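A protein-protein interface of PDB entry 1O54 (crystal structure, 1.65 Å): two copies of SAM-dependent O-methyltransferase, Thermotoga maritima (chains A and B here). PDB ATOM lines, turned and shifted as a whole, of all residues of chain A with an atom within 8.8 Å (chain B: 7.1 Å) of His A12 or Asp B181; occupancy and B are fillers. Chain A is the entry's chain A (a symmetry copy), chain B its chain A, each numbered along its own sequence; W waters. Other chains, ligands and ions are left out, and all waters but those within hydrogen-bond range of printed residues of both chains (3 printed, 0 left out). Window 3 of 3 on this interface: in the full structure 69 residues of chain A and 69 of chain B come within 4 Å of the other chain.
The side-chain carboxylate (OD1) of Asp B181 lies within hydrogen-bond range of a ring nitrogen (NE2) of His A12. The side-chain amino group (NZ) of Lys A15 lies within salt-bridge range of the side-chain carboxylate (OD1) of Asp B183. The side-chain amino group (NZ) of Lys B204 is in salt-bridge range of the side-chain carboxylate (OD2) of Asp A18, at 2.7 Å.
Hydrophobic or aromatic side chains of chain A within 4 Å of the printed part of chain B: His A12 and Pro A63. Of the 14 printed residues of chain B, 4 touch a printed residue of chain A. Printed residues of chain B that touch a printed residue of chain A: Asp B181, Asp B183, Lys B204 and Gly B205. Among the printed residues, 5 pairs touch across the chains. Among the printed residues, Asp or Glu carboxylates within 4 Å of a Lys or Arg side-chain nitrogen of the other chain: Lys A15 with Asp B183 and Asp A18 with Lys B204.
The backbone carbonyl oxygen (O) of Val B182 sits at hydrogen-bond distance from the backbone NH (N) of Lys B204, at 2.9 Å. The backbone NH (N) of Asp B181 lies within hydrogen-bond range of the backbone carbonyl oxygen (O) of Ala B202. NH1 of Arg B115 is in hydrogen-bond range of O of Asp B181 (3.3 Å). The side-chain carboxylate of Asp B183 lies within salt-bridge range of the side-chain amino group of Lys B204, at 2.8 Å. The backbone carbonyl oxygen of Arg B115 is in hydrogen-bond range of the backbone NH of Asp B183 (2.8 Å).
Water W1 bridges OD2 of Asp B181 (2.7 Å) and NE2 of His A12 (3.1 Å). Water W3 lies within hydrogen-bond range of OD2 of Asp A18 (2.7 Å) and O of Gly B205 (2.8 Å). Water W2 lies within hydrogen-bond range of NZ of Lys A15 and OD2 of Asp B183.
Among the printed residues, pairs that only touch across the chains: Gly A14 with Asp B181 and Pro A63 with Gly B205.
No position is printed for both chains. Of the 5 pairs that touch across the chains among the printed residues, none has its exchanged pair printed and touching as well.
His A12 touches just one residue of chain B: Asp B181 (2.7 Å). Of the printed residues of chain B, Gly A14 touches Asp B181 (3.5 Å). Of chain A, only His A12 and Gly A14 come within 4 Å of Asp B181. No residue of chain A comes within 4 Å of Val B182. Of the printed residues of chain A, Asp B183 touches Lys A15. Of the printed residues of chain A, Lys B204 touches Asp A18 (2.7 Å). Of the printed residues of chain A, Gly B205 touches Pro A63 (3.4 Å). The nearest residue of chain B that does not touch His A12 is Lys B180 (5.8 Å). The nearest residue of chain A that does not touch Asp B181 is Lys A15 (4.6 Å).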
ATOM      1  N   HIS A  10       1.960  -7.233   9.217  1.00  0.00           N
ATOM      2  CA  HIS A  10       0.743  -7.351   8.365  1.00  0.00           C
ATOM      3  C   HIS A  10      -0.049  -8.589   8.683  1.00  0.00           C
ATOM      4  O   HIS A  10       0.455  -9.535   9.295  1.00  0.00           O
ATOM      5  CB  HIS A  10       1.102  -7.338   6.879  1.00  0.00           C
ATOM      6  CG  HIS A  10       1.800  -8.575   6.403  1.00  0.00           C
ATOM      7  ND1 HIS A  10       3.173  -8.713   6.434  1.00  0.00           N
ATOM      8  CD2 HIS A  10       1.316  -9.713   5.848  1.00  0.00           C
ATOM      9  CE1 HIS A  10       3.500  -9.888   5.927  1.00  0.00           C
ATOM     10  NE2 HIS A  10       2.392 -10.516   5.569  1.00  0.00           N
ATOM     11  N   HIS A  11      -1.300  -8.562   8.251  1.00  0.00           N
ATOM     12  CA  HIS A  11      -2.212  -9.665   8.432  1.00  0.00           C
ATOM     13  C   HIS A  11      -1.859 -10.782   7.440  1.00  0.00           C
ATOM     14  O   HIS A  11      -1.908 -10.583   6.219  1.00  0.00           O
ATOM     15  CB  HIS A  11      -3.651  -9.167   8.191  1.00  0.00           C
ATOM     16  CG  HIS A  11      -4.657 -10.267   8.164  1.00  0.00           C
ATOM     17  ND1 HIS A  11      -5.090 -10.906   9.307  1.00  0.00           N
ATOM     18  CD2 HIS A  11      -5.286 -10.868   7.127  1.00  0.00           C
ATOM     19  CE1 HIS A  11      -5.941 -11.862   8.969  1.00  0.00           C
ATOM     20  NE2 HIS A  11      -6.094 -11.843   7.653  1.00  0.00           N
ATOM     21  N   HIS A  12      -1.543 -11.967   7.962  1.00  0.00           N
ATOM     22  CA  HIS A  12      -1.162 -13.106   7.137  1.00  0.00           C
ATOM     23  C   HIS A  12      -2.412 -13.965   6.843  1.00  0.00           C
ATOM     24  O   HIS A  12      -3.233 -14.229   7.736  1.00  0.00           O
ATOM     25  CB  HIS A  12      -0.077 -13.914   7.883  1.00  0.00           C
ATOM     26  CG  HIS A  12       0.481 -15.080   7.118  1.00  0.00           C
ATOM     27  ND1 HIS A  12       1.052 -14.964   5.866  1.00  0.00           N
ATOM     28  CD2 HIS A  12       0.610 -16.386   7.464  1.00  0.00           C
ATOM     29  CE1 HIS A  12       1.477 -16.151   5.464  1.00  0.00           C
ATOM     30  NE2 HIS A  12       1.214 -17.033   6.413  1.00  0.00           N
ATOM     31  N   VAL A  13      -2.556 -14.405   5.599  1.00  0.00           N
ATOM     32  CA  VAL A  13      -3.700 -15.227   5.218  1.00  0.00           C
ATOM     33  C   VAL A  13      -3.627 -16.572   5.956  1.00  0.00           C
ATOM     34  O   VAL A  13      -4.616 -17.022   6.575  1.00  0.00           O
ATOM     35  CB  VAL A  13      -3.772 -15.391   3.698  1.00  0.00           C
ATOM     36  CG1 VAL A  13      -4.804 -16.422   3.289  1.00  0.00           C
ATOM     37  CG2 VAL A  13      -4.093 -14.045   3.052  1.00  0.00           C
ATOM     38  N   GLY A  14      -2.465 -17.200   5.892  1.00  0.00           N
ATOM     39  CA  GLY A  14      -2.169 -18.365   6.735  1.00  0.00           C
ATOM     40  C   GLY A  14      -3.076 -19.532   6.476  1.00  0.00           C
ATOM     41  O   GLY A  14      -3.307 -19.887   5.315  1.00  0.00           O
ATOM     42  N   LYS A  15      -3.600 -20.126   7.557  1.00  0.00           N
ATOM     43  CA  LYS A  15      -4.516 -21.247   7.452  1.00  0.00           C
ATOM     44  C   LYS A  15      -5.958 -20.784   7.258  1.00  0.00           C
ATOM     45  O   LYS A  15      -6.579 -20.263   8.189  1.00  0.00           O
ATOM     46  CB  LYS A  15      -4.443 -22.137   8.697  1.00  0.00           C
ATOM     47  CG  LYS A  15      -5.437 -23.280   8.583  1.00  0.00           C
ATOM     48  CD  LYS A  15      -5.133 -24.383   9.499  1.00  0.00           C
ATOM     49  CE  LYS A  15      -6.048 -25.536   9.248  1.00  0.00           C
ATOM     50  NZ  LYS A  15      -5.673 -26.686  10.092  1.00  0.00           N
ATOM     51  N   VAL A  16      -6.510 -21.040   6.082  1.00  0.00           N
ATOM     52  CA  VAL A  16      -7.768 -20.422   5.702  1.00  0.00           C
ATOM     53  C   VAL A  16      -8.896 -20.913   6.568  1.00  0.00           C
ATOM     54  O   VAL A  16      -9.806 -20.151   6.890  1.00  0.00           O
ATOM     55  CB  VAL A  16      -8.064 -20.596   4.175  1.00  0.00           C
ATOM     56  CG1 VAL A  16      -9.521 -20.323   3.849  1.00  0.00           C
ATOM     57  CG2 VAL A  16      -7.160 -19.679   3.361  1.00  0.00           C
ATOM     58  N   ASP A  18      -8.922 -21.277   9.579  1.00  0.00           N
ATOM     59  CA  ASP A  18      -8.890 -20.518  10.843  1.00  0.00           C
ATOM     60  C   ASP A  18      -9.363 -19.065  10.699  1.00  0.00           C
ATOM     61  O   ASP A  18      -9.284 -18.308  11.653  1.00  0.00           O
ATOM     62  CB  ASP A  18      -7.471 -20.445  11.376  1.00  0.00           C
ATOM     63  CG  ASP A  18      -6.981 -21.743  11.994  1.00  0.00           C
ATOM     64  OD1 ASP A  18      -7.751 -22.726  12.073  1.00  0.00           O
ATOM     65  OD2 ASP A  18      -5.810 -21.807  12.422  1.00  0.00           O
ATOM     66  N   THR A  19      -9.821 -18.676   9.517  1.00  0.00           N
ATOM     67  CA  THR A  19     -10.336 -17.319   9.281  1.00  0.00           C
ATOM     68  C   THR A  19     -11.483 -16.987  10.241  1.00  0.00           C
ATOM     69  O   THR A  19     -12.388 -17.803  10.411  1.00  0.00           O
ATOM     70  CB  THR A  19     -10.815 -17.226   7.837  1.00  0.00           C
ATOM     71  OG1 THR A  19      -9.696 -17.408   6.959  1.00  0.00           O
ATOM     72  CG2 THR A  19     -11.353 -15.819   7.517  1.00  0.00           C
ATOM     73  N   GLU A  60     -11.220  -7.940  11.881  1.00  0.00           N
ATOM     74  CA  GLU A  60     -10.154  -7.313  11.064  1.00  0.00           C
ATOM     75  C   GLU A  60      -8.766  -7.770  11.445  1.00  0.00           C
ATOM     76  O   GLU A  60      -7.773  -7.140  11.034  1.00  0.00           O
ATOM     77  CB  GLU A  60     -10.201  -5.816  11.229  1.00  0.00           C
ATOM     78  CG  GLU A  60     -11.581  -5.216  11.144  1.00  0.00           C
ATOM     79  CD  GLU A  60     -12.254  -5.507   9.810  1.00  0.00           C
ATOM     80  OE1 GLU A  60     -11.787  -6.371   9.027  1.00  0.00           O
ATOM     81  OE2 GLU A  60     -13.257  -4.876   9.571  1.00  0.00           O
ATOM     82  N   LYS A  61      -8.710  -8.826  12.264  1.00  0.00           N
ATOM     83  CA  LYS A  61      -7.462  -9.387  12.752  1.00  0.00           C
ATOM     84  C   LYS A  61      -7.483 -10.868  12.411  1.00  0.00           C
ATOM     85  O   LYS A  61      -8.222 -11.294  11.514  1.00  0.00           O
ATOM     86  CB  LYS A  61      -7.338  -9.140  14.261  1.00  0.00           C
ATOM     87  CG  LYS A  61      -7.456  -7.673  14.691  1.00  0.00           C
ATOM     88  CD  LYS A  61      -6.120  -7.021  14.937  1.00  0.00           C
ATOM     89  CE  LYS A  61      -6.248  -5.723  15.746  1.00  0.00           C
ATOM     90  NZ  LYS A  61      -4.941  -5.393  16.392  1.00  0.00           N
ATOM     91  N   GLY A  62      -6.707 -11.681  13.110  1.00  0.00           N
ATOM     92  CA  GLY A  62      -6.549 -13.093  12.780  1.00  0.00           C
ATOM     93  C   GLY A  62      -5.928 -13.783  13.988  1.00  0.00           C
ATOM     94  O   GLY A  62      -5.489 -13.080  14.906  1.00  0.00           O
ATOM     95  N   PRO A  63      -5.893 -15.116  14.039  1.00  0.00           N
ATOM     96  CA  PRO A  63      -5.279 -15.781  15.166  1.00  0.00           C
ATOM     97  C   PRO A  63      -3.806 -15.412  15.285  1.00  0.00           C
ATOM     98  O   PRO A  63      -3.085 -15.344  14.266  1.00  0.00           O
ATOM     99  CB  PRO A  63      -5.471 -17.271  14.859  1.00  0.00           C
ATOM    100  CG  PRO A  63      -6.530 -17.301  13.872  1.00  0.00           C
ATOM    101  CD  PRO A  63      -6.438 -16.100  13.079  1.00  0.00           C
ATOM    102  N   GLU A  65      -2.801 -12.556  16.414  1.00  0.00           N
ATOM    103  CA  GLU A  65      -2.685 -11.098  16.419  1.00  0.00           C
ATOM    104  C   GLU A  65      -3.138 -10.478  17.745  1.00  0.00           C
ATOM    105  O   GLU A  65      -3.940 -11.048  18.484  1.00  0.00           O
ATOM    106  CB  GLU A  65      -3.485 -10.487  15.263  1.00  0.00           C
ATOM    107  CG  GLU A  65      -2.992 -10.885  13.889  1.00  0.00           C
ATOM    108  CD  GLU A  65      -3.744 -10.178  12.755  1.00  0.00           C
ATOM    109  OE1 GLU A  65      -4.149  -9.000  12.895  1.00  0.00           O
ATOM    110  OE2 GLU A  65      -3.931 -10.802  11.720  1.00  0.00           O
ATOM    111  N   ARG B 115      -1.912 -30.118   9.939  1.00  0.00           N
ATOM    112  CA  ARG B 115      -0.540 -30.290   9.480  1.00  0.00           C
ATOM    113  C   ARG B 115       0.364 -30.097  10.712  1.00  0.00           C
ATOM    114  O   ARG B 115       0.318 -29.040  11.377  1.00  0.00           O
ATOM    115  CB  ARG B 115      -0.203 -29.255   8.403  1.00  0.00           C
ATOM    116  CG  ARG B 115      -0.976 -29.519   7.097  1.00  0.00           C
ATOM    117  CD  ARG B 115      -1.052 -28.317   6.134  1.00  0.00           C
ATOM    118  NE  ARG B 115       0.275 -27.961   5.631  1.00  0.00           N
ATOM    119  CZ  ARG B 115       0.989 -26.888   6.008  1.00  0.00           C
ATOM    120  NH1 ARG B 115       0.534 -26.038   6.912  1.00  0.00           N
ATOM    121  NH2 ARG B 115       2.155 -26.651   5.443  1.00  0.00           N
ATOM    122  N   GLU B 179       7.854 -26.338   5.730  1.00  0.00           N
ATOM    123  CA  GLU B 179       6.437 -26.046   5.859  1.00  0.00           C
ATOM    124  C   GLU B 179       6.254 -24.757   6.652  1.00  0.00           C
ATOM    125  O   GLU B 179       7.001 -24.482   7.610  1.00  0.00           O
ATOM    126  CB  GLU B 179       5.706 -27.164   6.576  1.00  0.00           C
ATOM    127  CG  GLU B 179       5.767 -28.513   5.891  1.00  0.00           C
ATOM    128  CD  GLU B 179       7.125 -29.208   6.017  1.00  0.00           C
ATOM    129  OE1 GLU B 179       7.893 -28.932   6.971  1.00  0.00           O
ATOM    130  OE2 GLU B 179       7.396 -30.065   5.161  1.00  0.00           O
ATOM    131  N   LYS B 180       5.231 -23.991   6.262  1.00  0.00           N
ATOM    132  CA  LYS B 180       4.781 -22.840   7.007  1.00  0.00           C
ATOM    133  C   LYS B 180       3.337 -23.020   7.422  1.00  0.00           C
ATOM    134  O   LYS B 180       2.584 -23.829   6.867  1.00  0.00           O
ATOM    135  CB  LYS B 180       4.881 -21.565   6.158  1.00  0.00           C
ATOM    136  CG  LYS B 180       6.277 -21.208   5.730  1.00  0.00           C
ATOM    137  CD  LYS B 180       7.122 -20.747   6.894  1.00  0.00           C
ATOM    138  CE  LYS B 180       8.390 -20.014   6.403  1.00  0.00           C
ATOM    139  NZ  LYS B 180       9.659 -20.462   7.059  1.00  0.00           N
ATOM    140  N   ASP B 181       2.972 -22.232   8.411  1.00  0.00           N
ATOM    141  CA  ASP B 181       1.644 -22.183   8.918  1.00  0.00           C
ATOM    142  C   ASP B 181       1.136 -23.531   9.412  1.00  0.00           C
ATOM    143  O   ASP B 181      -0.058 -23.805   9.318  1.00  0.00           O
ATOM    144  CB  ASP B 181       0.719 -21.604   7.869  1.00  0.00           C
ATOM    145  CG  ASP B 181       0.994 -20.135   7.622  1.00  0.00           C
ATOM    146  OD1 ASP B 181       1.048 -19.763   6.457  1.00  0.00           O
ATOM    147  OD2 ASP B 181       1.162 -19.337   8.561  1.00  0.00           O
ATOM    148  N   VAL B 182       2.032 -24.347   9.977  1.00  0.00           N
ATOM    149  CA  VAL B 182       1.591 -25.639  10.508  1.00  0.00           C
ATOM    150  C   VAL B 182       0.778 -25.430  11.792  1.00  0.00           C
ATOM    151  O   VAL B 182       0.931 -24.407  12.497  1.00  0.00           O
ATOM    152  CB  VAL B 182       2.737 -26.671  10.692  1.00  0.00           C
ATOM    153  CG1 VAL B 182       3.518 -26.846   9.415  1.00  0.00           C
ATOM    154  CG2 VAL B 182       3.631 -26.310  11.884  1.00  0.00           C
ATOM    155  N   ASP B 183      -0.105 -26.376  12.078  1.00  0.00           N
ATOM    156  CA  ASP B 183      -1.038 -26.225  13.191  1.00  0.00           C
ATOM    157  C   ASP B 183      -0.366 -26.406  14.549  1.00  0.00           C
ATOM    158  O   ASP B 183      -0.719 -25.732  15.523  1.00  0.00           O
ATOM    159  CB  ASP B 183      -2.158 -27.205  13.021  1.00  0.00           C
ATOM    160  CG  ASP B 183      -2.963 -26.914  11.785  1.00  0.00           C
ATOM    161  OD1 ASP B 183      -3.793 -25.985  11.857  1.00  0.00           O
ATOM    162  OD2 ASP B 183      -2.791 -27.518  10.708  1.00  0.00           O
ATOM    163  N   ALA B 184       0.581 -27.340  14.605  1.00  0.00           N
ATOM    164  CA  ALA B 184       1.288 -27.657  15.849  1.00  0.00           C
ATOM    165  C   ALA B 184       2.627 -28.301  15.512  1.00  0.00           C
ATOM    166  O   ALA B 184       2.824 -28.796  14.392  1.00  0.00           O
ATOM    167  CB  ALA B 184       0.488 -28.574  16.713  1.00  0.00           C
ATOM    168  N   GLU B 201       9.069 -20.096  13.452  1.00  0.00           N
ATOM    169  CA  GLU B 201       8.871 -19.671  12.049  1.00  0.00           C
ATOM    170  C   GLU B 201       7.875 -20.554  11.296  1.00  0.00           C
ATOM    171  O   GLU B 201       7.157 -20.086  10.411  1.00  0.00           O
ATOM    172  CB  GLU B 201      10.205 -19.638  11.322  1.00  0.00           C
ATOM    173  CG  GLU B 201      11.089 -18.502  11.805  1.00  0.00           C
ATOM    174  CD  GLU B 201      12.541 -18.580  11.352  1.00  0.00           C
ATOM    175  OE1 GLU B 201      12.952 -19.569  10.681  1.00  0.00           O
ATOM    176  OE2 GLU B 201      13.277 -17.620  11.683  1.00  0.00           O
ATOM    177  N   ALA B 202       7.870 -21.834  11.627  1.00  0.00           N
ATOM    178  CA  ALA B 202       7.017 -22.818  10.935  1.00  0.00           C
ATOM    179  C   ALA B 202       5.549 -22.793  11.377  1.00  0.00           C
ATOM    180  O   ALA B 202       4.684 -23.231  10.628  1.00  0.00           O
ATOM    181  CB  ALA B 202       7.584 -24.210  11.108  1.00  0.00           C
ATOM    182  N   LEU B 203       5.275 -22.328  12.589  1.00  0.00           N
ATOM    183  CA  LEU B 203       3.926 -22.365  13.168  1.00  0.00           C
ATOM    184  C   LEU B 203       3.005 -21.282  12.634  1.00  0.00           C
ATOM    185  O   LEU B 203       3.449 -20.154  12.407  1.00  0.00           O
ATOM    186  CB  LEU B 203       4.016 -22.249  14.680  1.00  0.00           C
ATOM    187  CG  LEU B 203       4.512 -23.522  15.360  1.00  0.00           C
ATOM    188  CD1 LEU B 203       4.958 -23.263  16.738  1.00  0.00           C
ATOM    189  CD2 LEU B 203       3.379 -24.506  15.354  1.00  0.00           C
ATOM    190  N   LYS B 204       1.740 -21.620  12.426  1.00  0.00           N
ATOM    191  CA  LYS B 204       0.706 -20.602  12.156  1.00  0.00           C
ATOM    192  C   LYS B 204       0.517 -19.682  13.385  1.00  0.00           C
ATOM    193  O   LYS B 204       0.904 -20.032  14.509  1.00  0.00           O
ATOM    194  CB  LYS B 204      -0.625 -21.277  11.814  1.00  0.00           C
ATOM    195  CG  LYS B 204      -1.285 -21.979  12.967  1.00  0.00           C
ATOM    196  CD  LYS B 204      -2.588 -22.675  12.628  1.00  0.00           C
ATOM    197  CE  LYS B 204      -3.305 -23.142  13.882  1.00  0.00           C
ATOM    198  NZ  LYS B 204      -4.543 -23.921  13.596  1.00  0.00           N
ATOM    199  N   GLY B 205      -0.067 -18.509  13.153  1.00  0.00           N
ATOM    200  CA  GLY B 205      -0.548 -17.672  14.241  1.00  0.00           C
ATOM    201  C   GLY B 205      -1.504 -18.441  15.109  1.00  0.00           C
ATOM    202  O   GLY B 205      -2.480 -19.014  14.636  1.00  0.00           O
ATOM    203  N   LYS B 269       2.287 -19.853  19.695  1.00  0.00           N
ATOM    204  CA  LYS B 269       2.869 -18.824  18.855  1.00  0.00           C
ATOM    205  C   LYS B 269       1.927 -17.664  18.645  1.00  0.00           C
ATOM    206  O   LYS B 269       0.755 -17.842  18.288  1.00  0.00           O
ATOM    207  CB  LYS B 269       3.244 -19.400  17.494  1.00  0.00           C
ATOM    208  CG  LYS B 269       3.984 -18.392  16.559  1.00  0.00           C
ATOM    209  CD  LYS B 269       3.553 -18.494  15.219  1.00  0.00           C
ATOM    210  CE  LYS B 269       4.025 -17.397  14.303  1.00  0.00           C
ATOM    211  NZ  LYS B 269       4.932 -17.960  13.291  1.00  0.00           N
ATOM    212  N   CYS B 271       2.111 -13.579  16.629  1.00  0.00           N
ATOM    213  CA  CYS B 271       2.846 -12.944  15.535  1.00  0.00           C
ATOM    214  C   CYS B 271       3.936 -11.999  16.027  1.00  0.00           C
ATOM    215  O   CYS B 271       4.995 -11.911  15.417  1.00  0.00           O
ATOM    216  CB  CYS B 271       1.885 -12.212  14.597  1.00  0.00           C
ATOM    217  SG  CYS B 271       0.794 -13.419  13.799  1.00  0.00           S
HETATM  218  O   HOH W   1       3.498 -18.075   8.315  1.00  0.00           O
HETATM  219  O   HOH W   2      -4.213 -28.012   8.088  1.00  0.00           O
HETATM  220  O   HOH W   3      -4.132 -19.643  12.431  1.00  0.00           O
